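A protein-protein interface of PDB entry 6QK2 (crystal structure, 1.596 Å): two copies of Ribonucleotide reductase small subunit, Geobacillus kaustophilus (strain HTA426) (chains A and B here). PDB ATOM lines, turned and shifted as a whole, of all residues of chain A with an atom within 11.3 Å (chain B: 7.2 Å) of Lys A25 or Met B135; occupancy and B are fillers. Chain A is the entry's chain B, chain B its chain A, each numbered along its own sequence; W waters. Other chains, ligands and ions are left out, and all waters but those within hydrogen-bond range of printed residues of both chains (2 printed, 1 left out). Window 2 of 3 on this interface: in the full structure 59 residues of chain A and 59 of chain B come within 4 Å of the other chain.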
ATOM      1  N   HIS A  17     -14.564 -16.863   7.562  1.00  0.00           N
ATOM      2  CA  HIS A  17     -14.853 -16.872   6.140  1.00  0.00           C
ATOM      3  C   HIS A  17     -16.079 -16.022   5.816  1.00  0.00           C
ATOM      4  O   HIS A  17     -16.930 -15.743   6.667  1.00  0.00           O
ATOM      5  CB  HIS A  17     -15.054 -18.315   5.687  1.00  0.00           C
ATOM      6  CG  HIS A  17     -13.844 -19.177   5.894  1.00  0.00           C
ATOM      7  ND1 HIS A  17     -13.811 -20.516   5.557  1.00  0.00           N
ATOM      8  CD2 HIS A  17     -12.618 -18.884   6.395  1.00  0.00           C
ATOM      9  CE1 HIS A  17     -12.618 -21.011   5.847  1.00  0.00           C
ATOM     10  NE2 HIS A  17     -11.876 -20.042   6.358  1.00  0.00           N
ATOM     11  N   HIS A  18     -16.166 -15.610   4.558  1.00  0.00           N
ATOM     12  CA  HIS A  18     -17.365 -14.955   4.053  1.00  0.00           C
ATOM     13  C   HIS A  18     -18.287 -16.043   3.518  1.00  0.00           C
ATOM     14  O   HIS A  18     -17.839 -16.917   2.776  1.00  0.00           O
ATOM     15  CB  HIS A  18     -17.067 -13.959   2.923  1.00  0.00           C
ATOM     16  CG  HIS A  18     -16.160 -12.824   3.297  1.00  0.00           C
ATOM     17  ND1 HIS A  18     -16.551 -11.806   4.144  1.00  0.00           N
ATOM     18  CD2 HIS A  18     -14.899 -12.517   2.901  1.00  0.00           C
ATOM     19  CE1 HIS A  18     -15.561 -10.942   4.279  1.00  0.00           C
ATOM     20  NE2 HIS A  18     -14.553 -11.340   3.524  1.00  0.00           N
ATOM     21  N   ASP A  19     -19.570 -15.974   3.868  1.00  0.00           N
ATOM     22  CA  ASP A  19     -20.522 -16.980   3.386  1.00  0.00           C
ATOM     23  C   ASP A  19     -20.933 -16.716   1.944  1.00  0.00           C
ATOM     24  O   ASP A  19     -21.241 -17.645   1.187  1.00  0.00           O
ATOM     25  CB  ASP A  19     -21.747 -16.993   4.306  1.00  0.00           C
ATOM     26  CG  ASP A  19     -22.958 -17.609   3.656  1.00  0.00           C
ATOM     27  OD1 ASP A  19     -22.858 -18.779   3.221  1.00  0.00           O
ATOM     28  OD2 ASP A  19     -24.006 -16.920   3.584  1.00  0.00           O
ATOM     29  N   GLY A  20     -20.878 -15.459   1.556  1.00  0.00           N
ATOM     30  CA  GLY A  20     -21.343 -14.979   0.276  1.00  0.00           C
ATOM     31  C   GLY A  20     -21.339 -13.475   0.404  1.00  0.00           C
ATOM     32  O   GLY A  20     -20.947 -12.927   1.443  1.00  0.00           O
ATOM     33  N   PHE A  21     -21.787 -12.813  -0.657  1.00  0.00           N
ATOM     34  CA  PHE A  21     -21.720 -11.363  -0.724  1.00  0.00           C
ATOM     35  C   PHE A  21     -23.051 -10.802  -1.180  1.00  0.00           C
ATOM     36  O   PHE A  21     -23.615 -11.240  -2.193  1.00  0.00           O
ATOM     37  CB  PHE A  21     -20.574 -10.922  -1.648  1.00  0.00           C
ATOM     38  CG  PHE A  21     -19.218 -11.387  -1.160  1.00  0.00           C
ATOM     39  CD1 PHE A  21     -18.542 -10.672  -0.207  1.00  0.00           C
ATOM     40  CD2 PHE A  21     -18.666 -12.569  -1.629  1.00  0.00           C
ATOM     41  CE1 PHE A  21     -17.323 -11.096   0.245  1.00  0.00           C
ATOM     42  CE2 PHE A  21     -17.459 -13.006  -1.176  1.00  0.00           C
ATOM     43  CZ  PHE A  21     -16.780 -12.286  -0.239  1.00  0.00           C
ATOM     44  N   GLN A  22     -23.493  -9.753  -0.482  1.00  0.00           N
ATOM     45  CA  GLN A  22     -24.782  -9.148  -0.755  1.00  0.00           C
ATOM     46  C   GLN A  22     -24.859  -8.585  -2.170  1.00  0.00           C
ATOM     47  O   GLN A  22     -25.911  -8.658  -2.814  1.00  0.00           O
ATOM     48  CB  GLN A  22     -25.074  -8.053   0.269  1.00  0.00           C
ATOM     49  CG  GLN A  22     -26.438  -7.442   0.140  1.00  0.00           C
ATOM     50  CD  GLN A  22     -26.653  -6.336   1.160  1.00  0.00           C
ATOM     51  OE1 GLN A  22     -26.174  -6.414   2.299  1.00  0.00           O
ATOM     52  NE2 GLN A  22     -27.324  -5.287   0.745  1.00  0.00           N
ATOM     53  N   THR A  23     -23.784  -7.966  -2.657  1.00  0.00           N
ATOM     54  CA  THR A  23     -23.877  -7.330  -3.966  1.00  0.00           C
ATOM     55  C   THR A  23     -23.646  -8.320  -5.090  1.00  0.00           C
ATOM     56  O   THR A  23     -23.628  -7.924  -6.257  1.00  0.00           O
ATOM     57  CB  THR A  23     -22.910  -6.120  -4.079  1.00  0.00           C
ATOM     58  OG1 THR A  23     -21.540  -6.521  -3.956  1.00  0.00           O
ATOM     59  CG2 THR A  23     -23.252  -5.082  -3.033  1.00  0.00           C
ATOM     60  N   VAL A  24     -23.486  -9.597  -4.765  1.00  0.00           N
ATOM     61  CA  VAL A  24     -23.496 -10.673  -5.753  1.00  0.00           C
ATOM     62  C   VAL A  24     -24.836 -11.390  -5.760  1.00  0.00           C
ATOM     63  O   VAL A  24     -25.411 -11.651  -6.819  1.00  0.00           O
ATOM     64  CB  VAL A  24     -22.329 -11.642  -5.461  1.00  0.00           C
ATOM     65  CG1 VAL A  24     -22.401 -12.881  -6.314  1.00  0.00           C
ATOM     66  CG2 VAL A  24     -21.004 -10.938  -5.733  1.00  0.00           C
ATOM     67  N   LYS A  25     -25.352 -11.705  -4.577  1.00  0.00           N
ATOM     68  CA  LYS A  25     -26.662 -12.339  -4.465  1.00  0.00           C
ATOM     69  C   LYS A  25     -27.786 -11.381  -4.827  1.00  0.00           C
ATOM     70  O   LYS A  25     -28.824 -11.810  -5.357  1.00  0.00           O
ATOM     71  CB  LYS A  25     -26.848 -12.864  -3.052  1.00  0.00           C
ATOM     72  CG  LYS A  25     -25.943 -14.078  -2.758  1.00  0.00           C
ATOM     73  CD  LYS A  25     -25.560 -14.189  -1.287  1.00  0.00           C
ATOM     74  CE  LYS A  25     -26.743 -14.505  -0.387  1.00  0.00           C
ATOM     75  NZ  LYS A  25     -26.341 -14.533   1.067  1.00  0.00           N
ATOM     76  N   ALA A  26     -27.584 -10.078  -4.588  1.00  0.00           N
ATOM     77  CA  ALA A  26     -28.624  -9.067  -4.723  1.00  0.00           C
ATOM     78  C   ALA A  26     -27.960  -7.727  -5.008  1.00  0.00           C
ATOM     79  O   ALA A  26     -27.113  -7.660  -5.897  1.00  0.00           O
ATOM     80  CB  ALA A  26     -29.484  -8.993  -3.463  1.00  0.00           C
ATOM     81  N   THR A  27     -28.382  -6.659  -4.322  1.00  0.00           N
ATOM     82  CA  THR A  27     -27.767  -5.339  -4.465  1.00  0.00           C
ATOM     83  C   THR A  27     -27.675  -4.696  -3.092  1.00  0.00           C
ATOM     84  O   THR A  27     -28.246  -5.170  -2.114  1.00  0.00           O
ATOM     85  CB  THR A  27     -28.556  -4.385  -5.362  1.00  0.00           C
ATOM     86  OG1 THR A  27     -29.804  -4.072  -4.751  1.00  0.00           O
ATOM     87  CG2 THR A  27     -28.786  -4.988  -6.754  1.00  0.00           C
ATOM     88  N   ILE A  28     -26.964  -3.577  -3.046  1.00  0.00           N
ATOM     89  CA  ILE A  28     -27.132  -2.650  -1.935  1.00  0.00           C
ATOM     90  C   ILE A  28     -28.610  -2.401  -1.709  1.00  0.00           C
ATOM     91  O   ILE A  28     -29.391  -2.295  -2.665  1.00  0.00           O
ATOM     92  CB  ILE A  28     -26.377  -1.345  -2.245  1.00  0.00           C
ATOM     93  CG1 ILE A  28     -24.865  -1.567  -2.261  1.00  0.00           C
ATOM     94  CG2 ILE A  28     -26.825  -0.211  -1.290  1.00  0.00           C
ATOM     95  CD1 ILE A  28     -24.103  -0.353  -2.730  1.00  0.00           C
ATOM     96  N   ASP A  29     -29.012  -2.313  -0.428  1.00  0.00           N
ATOM     97  CA  ASP A  29     -30.367  -1.885  -0.071  1.00  0.00           C
ATOM     98  C   ASP A  29     -30.448  -0.381  -0.244  1.00  0.00           C
ATOM     99  O   ASP A  29     -30.117   0.402   0.662  1.00  0.00           O
ATOM    100  CB  ASP A  29     -30.738  -2.291   1.347  1.00  0.00           C
ATOM    101  CG  ASP A  29     -32.162  -1.829   1.757  1.00  0.00           C
ATOM    102  OD1 ASP A  29     -32.915  -1.214   0.954  1.00  0.00           O
ATOM    103  OD2 ASP A  29     -32.516  -2.059   2.936  1.00  0.00           O
ATOM    104  N   TRP A  30     -30.898   0.037  -1.434  1.00  0.00           N
ATOM    105  CA  TRP A  30     -30.902   1.446  -1.804  1.00  0.00           C
ATOM    106  C   TRP A  30     -31.794   2.306  -0.913  1.00  0.00           C
ATOM    107  O   TRP A  30     -31.582   3.525  -0.848  1.00  0.00           O
ATOM    108  CB  TRP A  30     -31.345   1.600  -3.278  1.00  0.00           C
ATOM    109  CG  TRP A  30     -30.628   0.692  -4.221  1.00  0.00           C
ATOM    110  CD1 TRP A  30     -31.163  -0.359  -4.919  1.00  0.00           C
ATOM    111  CD2 TRP A  30     -29.241   0.747  -4.588  1.00  0.00           C
ATOM    112  NE1 TRP A  30     -30.218  -0.947  -5.698  1.00  0.00           N
ATOM    113  CE2 TRP A  30     -29.015  -0.293  -5.522  1.00  0.00           C
ATOM    114  CE3 TRP A  30     -28.183   1.594  -4.246  1.00  0.00           C
ATOM    115  CZ2 TRP A  30     -27.765  -0.535  -6.096  1.00  0.00           C
ATOM    116  CZ3 TRP A  30     -26.912   1.336  -4.803  1.00  0.00           C
ATOM    117  CH2 TRP A  30     -26.729   0.287  -5.733  1.00  0.00           C
ATOM    118  N   GLN A 100     -22.040  -8.475  11.374  1.00  0.00           N
ATOM    119  CA  GLN A 100     -23.487  -8.639  11.366  1.00  0.00           C
ATOM    120  C   GLN A 100     -24.106  -8.508   9.976  1.00  0.00           C
ATOM    121  O   GLN A 100     -25.337  -8.601   9.865  1.00  0.00           O
ATOM    122  CB  GLN A 100     -24.125  -7.626  12.317  1.00  0.00           C
ATOM    123  CG  GLN A 100     -23.757  -7.889  13.787  1.00  0.00           C
ATOM    124  CD  GLN A 100     -24.431  -6.974  14.743  1.00  0.00           C
ATOM    125  OE1 GLN A 100     -25.259  -6.169  14.360  1.00  0.00           O
ATOM    126  NE2 GLN A 100     -24.078  -7.092  16.023  1.00  0.00           N
ATOM    127  N   GLY A 101     -23.307  -8.279   8.940  1.00  0.00           N
ATOM    128  CA  GLY A 101     -23.815  -8.159   7.581  1.00  0.00           C
ATOM    129  C   GLY A 101     -24.525  -6.862   7.253  1.00  0.00           C
ATOM    130  O   GLY A 101     -25.265  -6.783   6.257  1.00  0.00           O
ATOM    131  N   LEU A 103     -24.262  -4.029   5.634  1.00  0.00           N
ATOM    132  CA  LEU A 103     -23.391  -3.455   4.613  1.00  0.00           C
ATOM    133  C   LEU A 103     -23.592  -1.950   4.487  1.00  0.00           C
ATOM    134  O   LEU A 103     -22.616  -1.204   4.354  1.00  0.00           O
ATOM    135  CB  LEU A 103     -23.637  -4.108   3.272  1.00  0.00           C
ATOM    136  CG  LEU A 103     -22.741  -3.588   2.132  1.00  0.00           C
ATOM    137  CD1 LEU A 103     -21.235  -3.650   2.371  1.00  0.00           C
ATOM    138  CD2 LEU A 103     -23.095  -4.340   0.855  1.00  0.00           C
ATOM    139  N   GLU A 104     -24.838  -1.491   4.511  1.00  0.00           N
ATOM    140  CA  GLU A 104     -25.095  -0.063   4.320  1.00  0.00           C
ATOM    141  C   GLU A 104     -24.580   0.747   5.501  1.00  0.00           C
ATOM    142  O   GLU A 104     -24.064   1.844   5.299  1.00  0.00           O
ATOM    143  CB  GLU A 104     -26.583   0.183   4.105  1.00  0.00           C
ATOM    144  CG  GLU A 104     -27.115  -0.453   2.804  1.00  0.00           C
ATOM    145  CD  GLU A 104     -27.392  -1.951   2.935  1.00  0.00           C
ATOM    146  OE1 GLU A 104     -27.539  -2.482   4.079  1.00  0.00           O
ATOM    147  OE2 GLU A 104     -27.386  -2.620   1.866  1.00  0.00           O
ATOM    148  N   PHE B  61     -27.199  -3.426 -22.549  1.00  0.00           N
ATOM    149  CA  PHE B  61     -27.425  -4.757 -22.008  1.00  0.00           C
ATOM    150  C   PHE B  61     -28.712  -5.332 -22.571  1.00  0.00           C
ATOM    151  O   PHE B  61     -28.759  -6.513 -22.922  1.00  0.00           O
ATOM    152  CB  PHE B  61     -27.468  -4.703 -20.471  1.00  0.00           C
ATOM    153  CG  PHE B  61     -27.293  -6.025 -19.814  1.00  0.00           C
ATOM    154  CD1 PHE B  61     -26.031  -6.568 -19.664  1.00  0.00           C
ATOM    155  CD2 PHE B  61     -28.383  -6.719 -19.310  1.00  0.00           C
ATOM    156  CE1 PHE B  61     -25.849  -7.803 -19.033  1.00  0.00           C
ATOM    157  CE2 PHE B  61     -28.213  -7.960 -18.673  1.00  0.00           C
ATOM    158  CZ  PHE B  61     -26.950  -8.506 -18.544  1.00  0.00           C
ATOM    159  N   LYS B  69     -25.578 -11.504 -23.137  1.00  0.00           N
ATOM    160  CA  LYS B  69     -25.765 -10.935 -21.804  1.00  0.00           C
ATOM    161  C   LYS B  69     -24.884 -11.634 -20.782  1.00  0.00           C
ATOM    162  O   LYS B  69     -24.128 -10.984 -20.052  1.00  0.00           O
ATOM    163  CB  LYS B  69     -27.227 -11.030 -21.370  1.00  0.00           C
ATOM    164  CG  LYS B  69     -28.159 -10.070 -22.037  1.00  0.00           C
ATOM    165  CD  LYS B  69     -29.554 -10.289 -21.487  1.00  0.00           C
ATOM    166  CE  LYS B  69     -30.442  -9.093 -21.694  1.00  0.00           C
ATOM    167  NZ  LYS B  69     -30.843  -8.957 -23.094  1.00  0.00           N
ATOM    168  N   ILE B  70     -24.980 -12.964 -20.696  1.00  0.00           N
ATOM    169  CA  ILE B  70     -24.285 -13.665 -19.625  1.00  0.00           C
ATOM    170  C   ILE B  70     -22.783 -13.684 -19.851  1.00  0.00           C
ATOM    171  O   ILE B  70     -22.027 -13.912 -18.901  1.00  0.00           O
ATOM    172  CB  ILE B  70     -24.820 -15.100 -19.453  1.00  0.00           C
ATOM    173  CG1 ILE B  70     -24.459 -15.964 -20.663  1.00  0.00           C
ATOM    174  CG2 ILE B  70     -26.339 -15.074 -19.217  1.00  0.00           C
ATOM    175  CD1 ILE B  70     -24.857 -17.424 -20.510  1.00  0.00           C
ATOM    176  N   LEU B  73     -21.174 -11.404 -17.426  1.00  0.00           N
ATOM    177  CA  LEU B  73     -21.465 -11.414 -15.995  1.00  0.00           C
ATOM    178  C   LEU B  73     -20.412 -12.069 -15.111  1.00  0.00           C
ATOM    179  O   LEU B  73     -20.324 -11.686 -13.941  1.00  0.00           O
ATOM    180  CB  LEU B  73     -22.812 -12.079 -15.736  1.00  0.00           C
ATOM    181  CG  LEU B  73     -23.953 -11.401 -16.487  1.00  0.00           C
ATOM    182  CD1 LEU B  73     -25.213 -12.050 -16.090  1.00  0.00           C
ATOM    183  CD2 LEU B  73     -24.016  -9.887 -16.210  1.00  0.00           C
ATOM    184  N   GLU B  84     -16.609  -5.926  -2.298  1.00  0.00           N
ATOM    185  CA  GLU B  84     -17.272  -6.074  -1.018  1.00  0.00           C
ATOM    186  C   GLU B  84     -16.338  -6.726  -0.002  1.00  0.00           C
ATOM    187  O   GLU B  84     -16.223  -6.256   1.135  1.00  0.00           O
ATOM    188  CB  GLU B  84     -18.560  -6.868  -1.220  1.00  0.00           C
ATOM    189  CG  GLU B  84     -19.438  -6.947   0.038  1.00  0.00           C
ATOM    190  CD  GLU B  84     -20.824  -7.546  -0.217  1.00  0.00           C
ATOM    191  OE1 GLU B  84     -21.345  -7.476  -1.378  1.00  0.00           O
ATOM    192  OE2 GLU B  84     -21.406  -8.059   0.766  1.00  0.00           O
ATOM    193  N   GLN B 127     -25.211  -3.188 -11.853  1.00  0.00           N
ATOM    194  CA  GLN B 127     -26.105  -4.353 -11.842  1.00  0.00           C
ATOM    195  C   GLN B 127     -27.565  -3.940 -11.739  1.00  0.00           C
ATOM    196  O   GLN B 127     -28.435  -4.471 -12.448  1.00  0.00           O
ATOM    197  CB  GLN B 127     -25.758  -5.289 -10.683  1.00  0.00           C
ATOM    198  CG  GLN B 127     -24.457  -6.036 -10.814  1.00  0.00           C
ATOM    199  CD  GLN B 127     -24.386  -7.153  -9.769  1.00  0.00           C
ATOM    200  OE1 GLN B 127     -25.354  -7.908  -9.591  1.00  0.00           O
ATOM    201  NE2 GLN B 127     -23.276  -7.232  -9.047  1.00  0.00           N
ATOM    202  N   GLY B 131     -30.517  -4.325 -14.950  1.00  0.00           N
ATOM    203  CA  GLY B 131     -31.599  -5.252 -14.695  1.00  0.00           C
ATOM    204  C   GLY B 131     -31.231  -6.624 -14.165  1.00  0.00           C
ATOM    205  O   GLY B 131     -32.071  -7.536 -14.253  1.00  0.00           O
ATOM    206  N   ILE B 132     -30.034  -6.810 -13.589  1.00  0.00           N
ATOM    207  CA  ILE B 132     -29.602  -8.094 -13.063  1.00  0.00           C
ATOM    208  C   ILE B 132     -29.408  -8.065 -11.556  1.00  0.00           C
ATOM    209  O   ILE B 132     -28.822  -8.990 -10.994  1.00  0.00           O
ATOM    210  CB  ILE B 132     -28.314  -8.599 -13.751  1.00  0.00           C
ATOM    211  CG1 ILE B 132     -27.124  -7.672 -13.491  1.00  0.00           C
ATOM    212  CG2 ILE B 132     -28.559  -8.782 -15.239  1.00  0.00           C
ATOM    213  CD1 ILE B 132     -25.826  -8.218 -13.971  1.00  0.00           C
ATOM    214  N   GLY B 133     -29.897  -7.029 -10.886  1.00  0.00           N
ATOM    215  CA  GLY B 133     -29.778  -6.990  -9.434  1.00  0.00           C
ATOM    216  C   GLY B 133     -30.372  -8.201  -8.765  1.00  0.00           C
ATOM    217  O   GLY B 133     -29.875  -8.664  -7.730  1.00  0.00           O
ATOM    218  N   GLN B 134     -31.429  -8.755  -9.357  1.00  0.00           N
ATOM    219  CA  GLN B 134     -32.101  -9.906  -8.783  1.00  0.00           C
ATOM    220  C   GLN B 134     -31.381 -11.223  -9.065  1.00  0.00           C
ATOM    221  O   GLN B 134     -31.704 -12.236  -8.440  1.00  0.00           O
ATOM    222  CB  GLN B 134     -33.558  -9.940  -9.303  1.00  0.00           C
ATOM    223  CG  GLN B 134     -33.750 -10.359 -10.782  1.00  0.00           C
ATOM    224  CD  GLN B 134     -33.287  -9.338 -11.843  1.00  0.00           C
ATOM    225  OE1 GLN B 134     -33.127  -8.133 -11.585  1.00  0.00           O
ATOM    226  NE2 GLN B 134     -33.110  -9.826 -13.071  1.00  0.00           N
ATOM    227  N   MET B 135     -30.412 -11.238  -9.969  1.00  0.00           N
ATOM    228  CA  MET B 135     -29.736 -12.472 -10.339  1.00  0.00           C
ATOM    229  C   MET B 135     -28.609 -12.800  -9.357  1.00  0.00           C
ATOM    230  O   MET B 135     -27.840 -11.923  -8.953  1.00  0.00           O
ATOM    231  CB  MET B 135     -29.211 -12.334 -11.763  1.00  0.00           C
ATOM    232  CG  MET B 135     -28.565 -13.564 -12.344  1.00  0.00           C
ATOM    233  SD  MET B 135     -27.865 -13.157 -13.974  1.00  0.00           S
ATOM    234  CE  MET B 135     -29.046 -11.974 -14.572  1.00  0.00           C
ATOM    235  N   ASP B 136     -28.512 -14.071  -8.956  1.00  0.00           N
ATOM    236  CA  ASP B 136     -27.446 -14.501  -8.051  1.00  0.00           C
ATOM    237  C   ASP B 136     -26.217 -14.847  -8.873  1.00  0.00           C
ATOM    238  O   ASP B 136     -26.138 -15.920  -9.479  1.00  0.00           O
ATOM    239  CB  ASP B 136     -27.885 -15.685  -7.198  1.00  0.00           C
ATOM    240  CG  ASP B 136     -26.855 -16.070  -6.146  1.00  0.00           C
ATOM    241  OD1 ASP B 136     -25.705 -15.551  -6.169  1.00  0.00           O
ATOM    242  OD2 ASP B 136     -27.212 -16.896  -5.264  1.00  0.00           O
ATOM    243  N   LEU B 137     -25.242 -13.934  -8.884  1.00  0.00           N
ATOM    244  CA  LEU B 137     -24.038 -14.124  -9.676  1.00  0.00           C
ATOM    245  C   LEU B 137     -23.007 -15.017  -8.984  1.00  0.00           C
ATOM    246  O   LEU B 137     -21.927 -15.236  -9.543  1.00  0.00           O
ATOM    247  CB  LEU B 137     -23.450 -12.748 -10.021  1.00  0.00           C
ATOM    248  CG  LEU B 137     -24.372 -11.785 -10.777  1.00  0.00           C
ATOM    249  CD1 LEU B 137     -23.609 -10.495 -11.116  1.00  0.00           C
ATOM    250  CD2 LEU B 137     -24.962 -12.389 -12.040  1.00  0.00           C
ATOM    251  N   SER B 138     -23.325 -15.566  -7.800  1.00  0.00           N
ATOM    252  CA  SER B 138     -22.398 -16.445  -7.087  1.00  0.00           C
ATOM    253  C   SER B 138     -22.044 -17.693  -7.872  1.00  0.00           C
ATOM    254  O   SER B 138     -21.024 -18.335  -7.567  1.00  0.00           O
ATOM    255  CB  SER B 138     -22.998 -16.890  -5.749  1.00  0.00           C
ATOM    256  OG  SER B 138     -23.267 -15.760  -4.921  1.00  0.00           O
ATOM    257  N   VAL B 139     -22.870 -18.040  -8.867  1.00  0.00           N
ATOM    258  CA  VAL B 139     -22.632 -19.204  -9.714  1.00  0.00           C
ATOM    259  C   VAL B 139     -21.333 -19.081 -10.509  1.00  0.00           C
ATOM    260  O   VAL B 139     -20.793 -20.091 -10.968  1.00  0.00           O
ATOM    261  CB  VAL B 139     -23.852 -19.404 -10.647  1.00  0.00           C
ATOM    262  CG1 VAL B 139     -25.142 -19.490  -9.837  1.00  0.00           C
ATOM    263  CG2 VAL B 139     -23.963 -18.266 -11.651  1.00  0.00           C
ATOM    264  N   PHE B 140     -20.791 -17.870 -10.658  1.00  0.00           N
ATOM    265  CA  PHE B 140     -19.539 -17.666 -11.377  1.00  0.00           C
ATOM    266  C   PHE B 140     -18.318 -17.591 -10.460  1.00  0.00           C
ATOM    267  O   PHE B 140     -17.237 -17.173 -10.906  1.00  0.00           O
ATOM    268  CB  PHE B 140     -19.641 -16.412 -12.232  1.00  0.00           C
ATOM    269  CG  PHE B 140     -20.730 -16.473 -13.251  1.00  0.00           C
ATOM    270  CD1 PHE B 140     -20.723 -17.466 -14.215  1.00  0.00           C
ATOM    271  CD2 PHE B 140     -21.758 -15.559 -13.245  1.00  0.00           C
ATOM    272  CE1 PHE B 140     -21.731 -17.525 -15.167  1.00  0.00           C
ATOM    273  CE2 PHE B 140     -22.764 -15.607 -14.191  1.00  0.00           C
ATOM    274  CZ  PHE B 140     -22.756 -16.603 -15.151  1.00  0.00           C
ATOM    275  N   TYR B 150     -13.302 -15.843  -0.347  1.00  0.00           N
ATOM    276  CA  TYR B 150     -14.149 -16.270   0.757  1.00  0.00           C
ATOM    277  C   TYR B 150     -13.346 -16.739   1.949  1.00  0.00           C
ATOM    278  O   TYR B 150     -13.866 -16.711   3.065  1.00  0.00           O
ATOM    279  CB  TYR B 150     -15.074 -17.416   0.335  1.00  0.00           C
ATOM    280  CG  TYR B 150     -16.192 -17.101  -0.644  1.00  0.00           C
ATOM    281  CD1 TYR B 150     -17.472 -17.538  -0.378  1.00  0.00           C
ATOM    282  CD2 TYR B 150     -15.975 -16.429  -1.865  1.00  0.00           C
ATOM    283  CE1 TYR B 150     -18.510 -17.326  -1.254  1.00  0.00           C
ATOM    284  CE2 TYR B 150     -17.023 -16.205  -2.755  1.00  0.00           C
ATOM    285  CZ  TYR B 150     -18.295 -16.646  -2.437  1.00  0.00           C
ATOM    286  OH  TYR B 150     -19.365 -16.467  -3.293  1.00  0.00           O
HETATM  287  O   HOH W   1     -21.770 -14.672  -2.875  1.00  0.00           O
HETATM  288  O   HOH W   2     -25.248  -5.790  -6.885  1.00  0.00           O
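Among the printed residues, merely in contact across the chains: Val A24 with Ser B138, His A17 with Tyr B150, Thr A27 with Gly B133, Phe A21 with Glu B84, Phe A21 with Tyr B150, Asp A19 with Tyr B150, Val A24 with Asp B136, Lys A25 with Asp B136, Lys A25 with Met B135, Lys A25 with Ser B138 and Gly A20 with Tyr B150.
The side-chain carboxylate (OE2) of Glu B84 sits at hydrogen-bond distance from the backbone NH (N) of Gln A22 (3.0 Å). OG1 of Thr A23 lies within hydrogen-bond range of OE1 of Glu B84 (2.8 Å). The side-chain amide nitrogen (NE2) of Gln B127 lies within hydrogen-bond range of the backbone carbonyl oxygen (O) of Thr A23, 2.9 Å away. O of Val A24 sits at hydrogen-bond distance from N of Leu B137, 3.1 Å away. The backbone carbonyl oxygen (O) of Tyr B150 sits at hydrogen-bond distance from the backbone NH (N) of His A18. The backbone carbonyl oxygen (O) of Val A24 sits close to the backbone carbonyl oxygen (O) of Met B135, 3.2 Å away. O of Gly B133 sits close to O of Ala A26 (3.5 Å).
No position is printed for both chains. Of the 18 pairs that touch across the chains among the printed residues, none has its exchanged pair printed and touching as well.
Hydrophobic or aromatic side chains of chain A within 4 Å of the printed part of chain B: His A17, Phe A21 and Val A24.
The backbone carbonyl oxygen (O) of Gln B127 is in hydrogen-bond range of the backbone NH (N) of Ile B132 (3.1 Å). O of Gln B127 is in hydrogen-bond range of N of Gly B133, 3.3 Å away. The side-chain carboxylate (OD1) of Asp B136 sits at hydrogen-bond distance from the side-chain hydroxyl (OG) of Ser B138 (2.7 Å). The backbone carbonyl oxygen (O) of Thr A27 is in hydrogen-bond range of the side-chain amide nitrogen (NE2) of Gln A22, at 3.0 Å. NE2 of Gln A22 sits at hydrogen-bond distance from OE2 of Glu A104 (2.9 Å). The indole nitrogen (NE1) of Trp A30 sits at hydrogen-bond distance from the side-chain hydroxyl (OG1) of Thr A27, at 3.3 Å.
Water W2 lies within hydrogen-bond range of O of Thr A23 (2.8 Å), O of Ala A26 (2.8 Å) and NE2 of Gln B127 (3.3 Å). Water W1 lies within hydrogen-bond range of the side-chain hydroxyl (OG) of Ser B138 (2.8 Å), the backbone NH (N) of Phe A21 (2.9 Å) and the side-chain hydroxyl (OH) of Tyr B150 (3.0 Å).
Lys A25 touches three residues of chain B. No residue of chain A comes within 4 Å of Ile B132. Printed residues of chain A within 4 Å of Gly B133: Ala A26 (3.3 Å) and Thr A27 (3.5 Å). No residue of chain A comes within 4 Å of Gln B134. Leu B137 touches just one residue of chain A: Val A24. Printed residues of chain B within 4 Å of Gln A22: Glu B84. Of the printed residues of chain B, Gly A20 touches Tyr B150 (3.98 Å). Gly A101 touches none of the printed residues of chain B. Phe B61 touches none of the printed residues of chain A. The nearest residue of chain B that does not touch Lys A25 is Gly B133 (4.1 Å).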
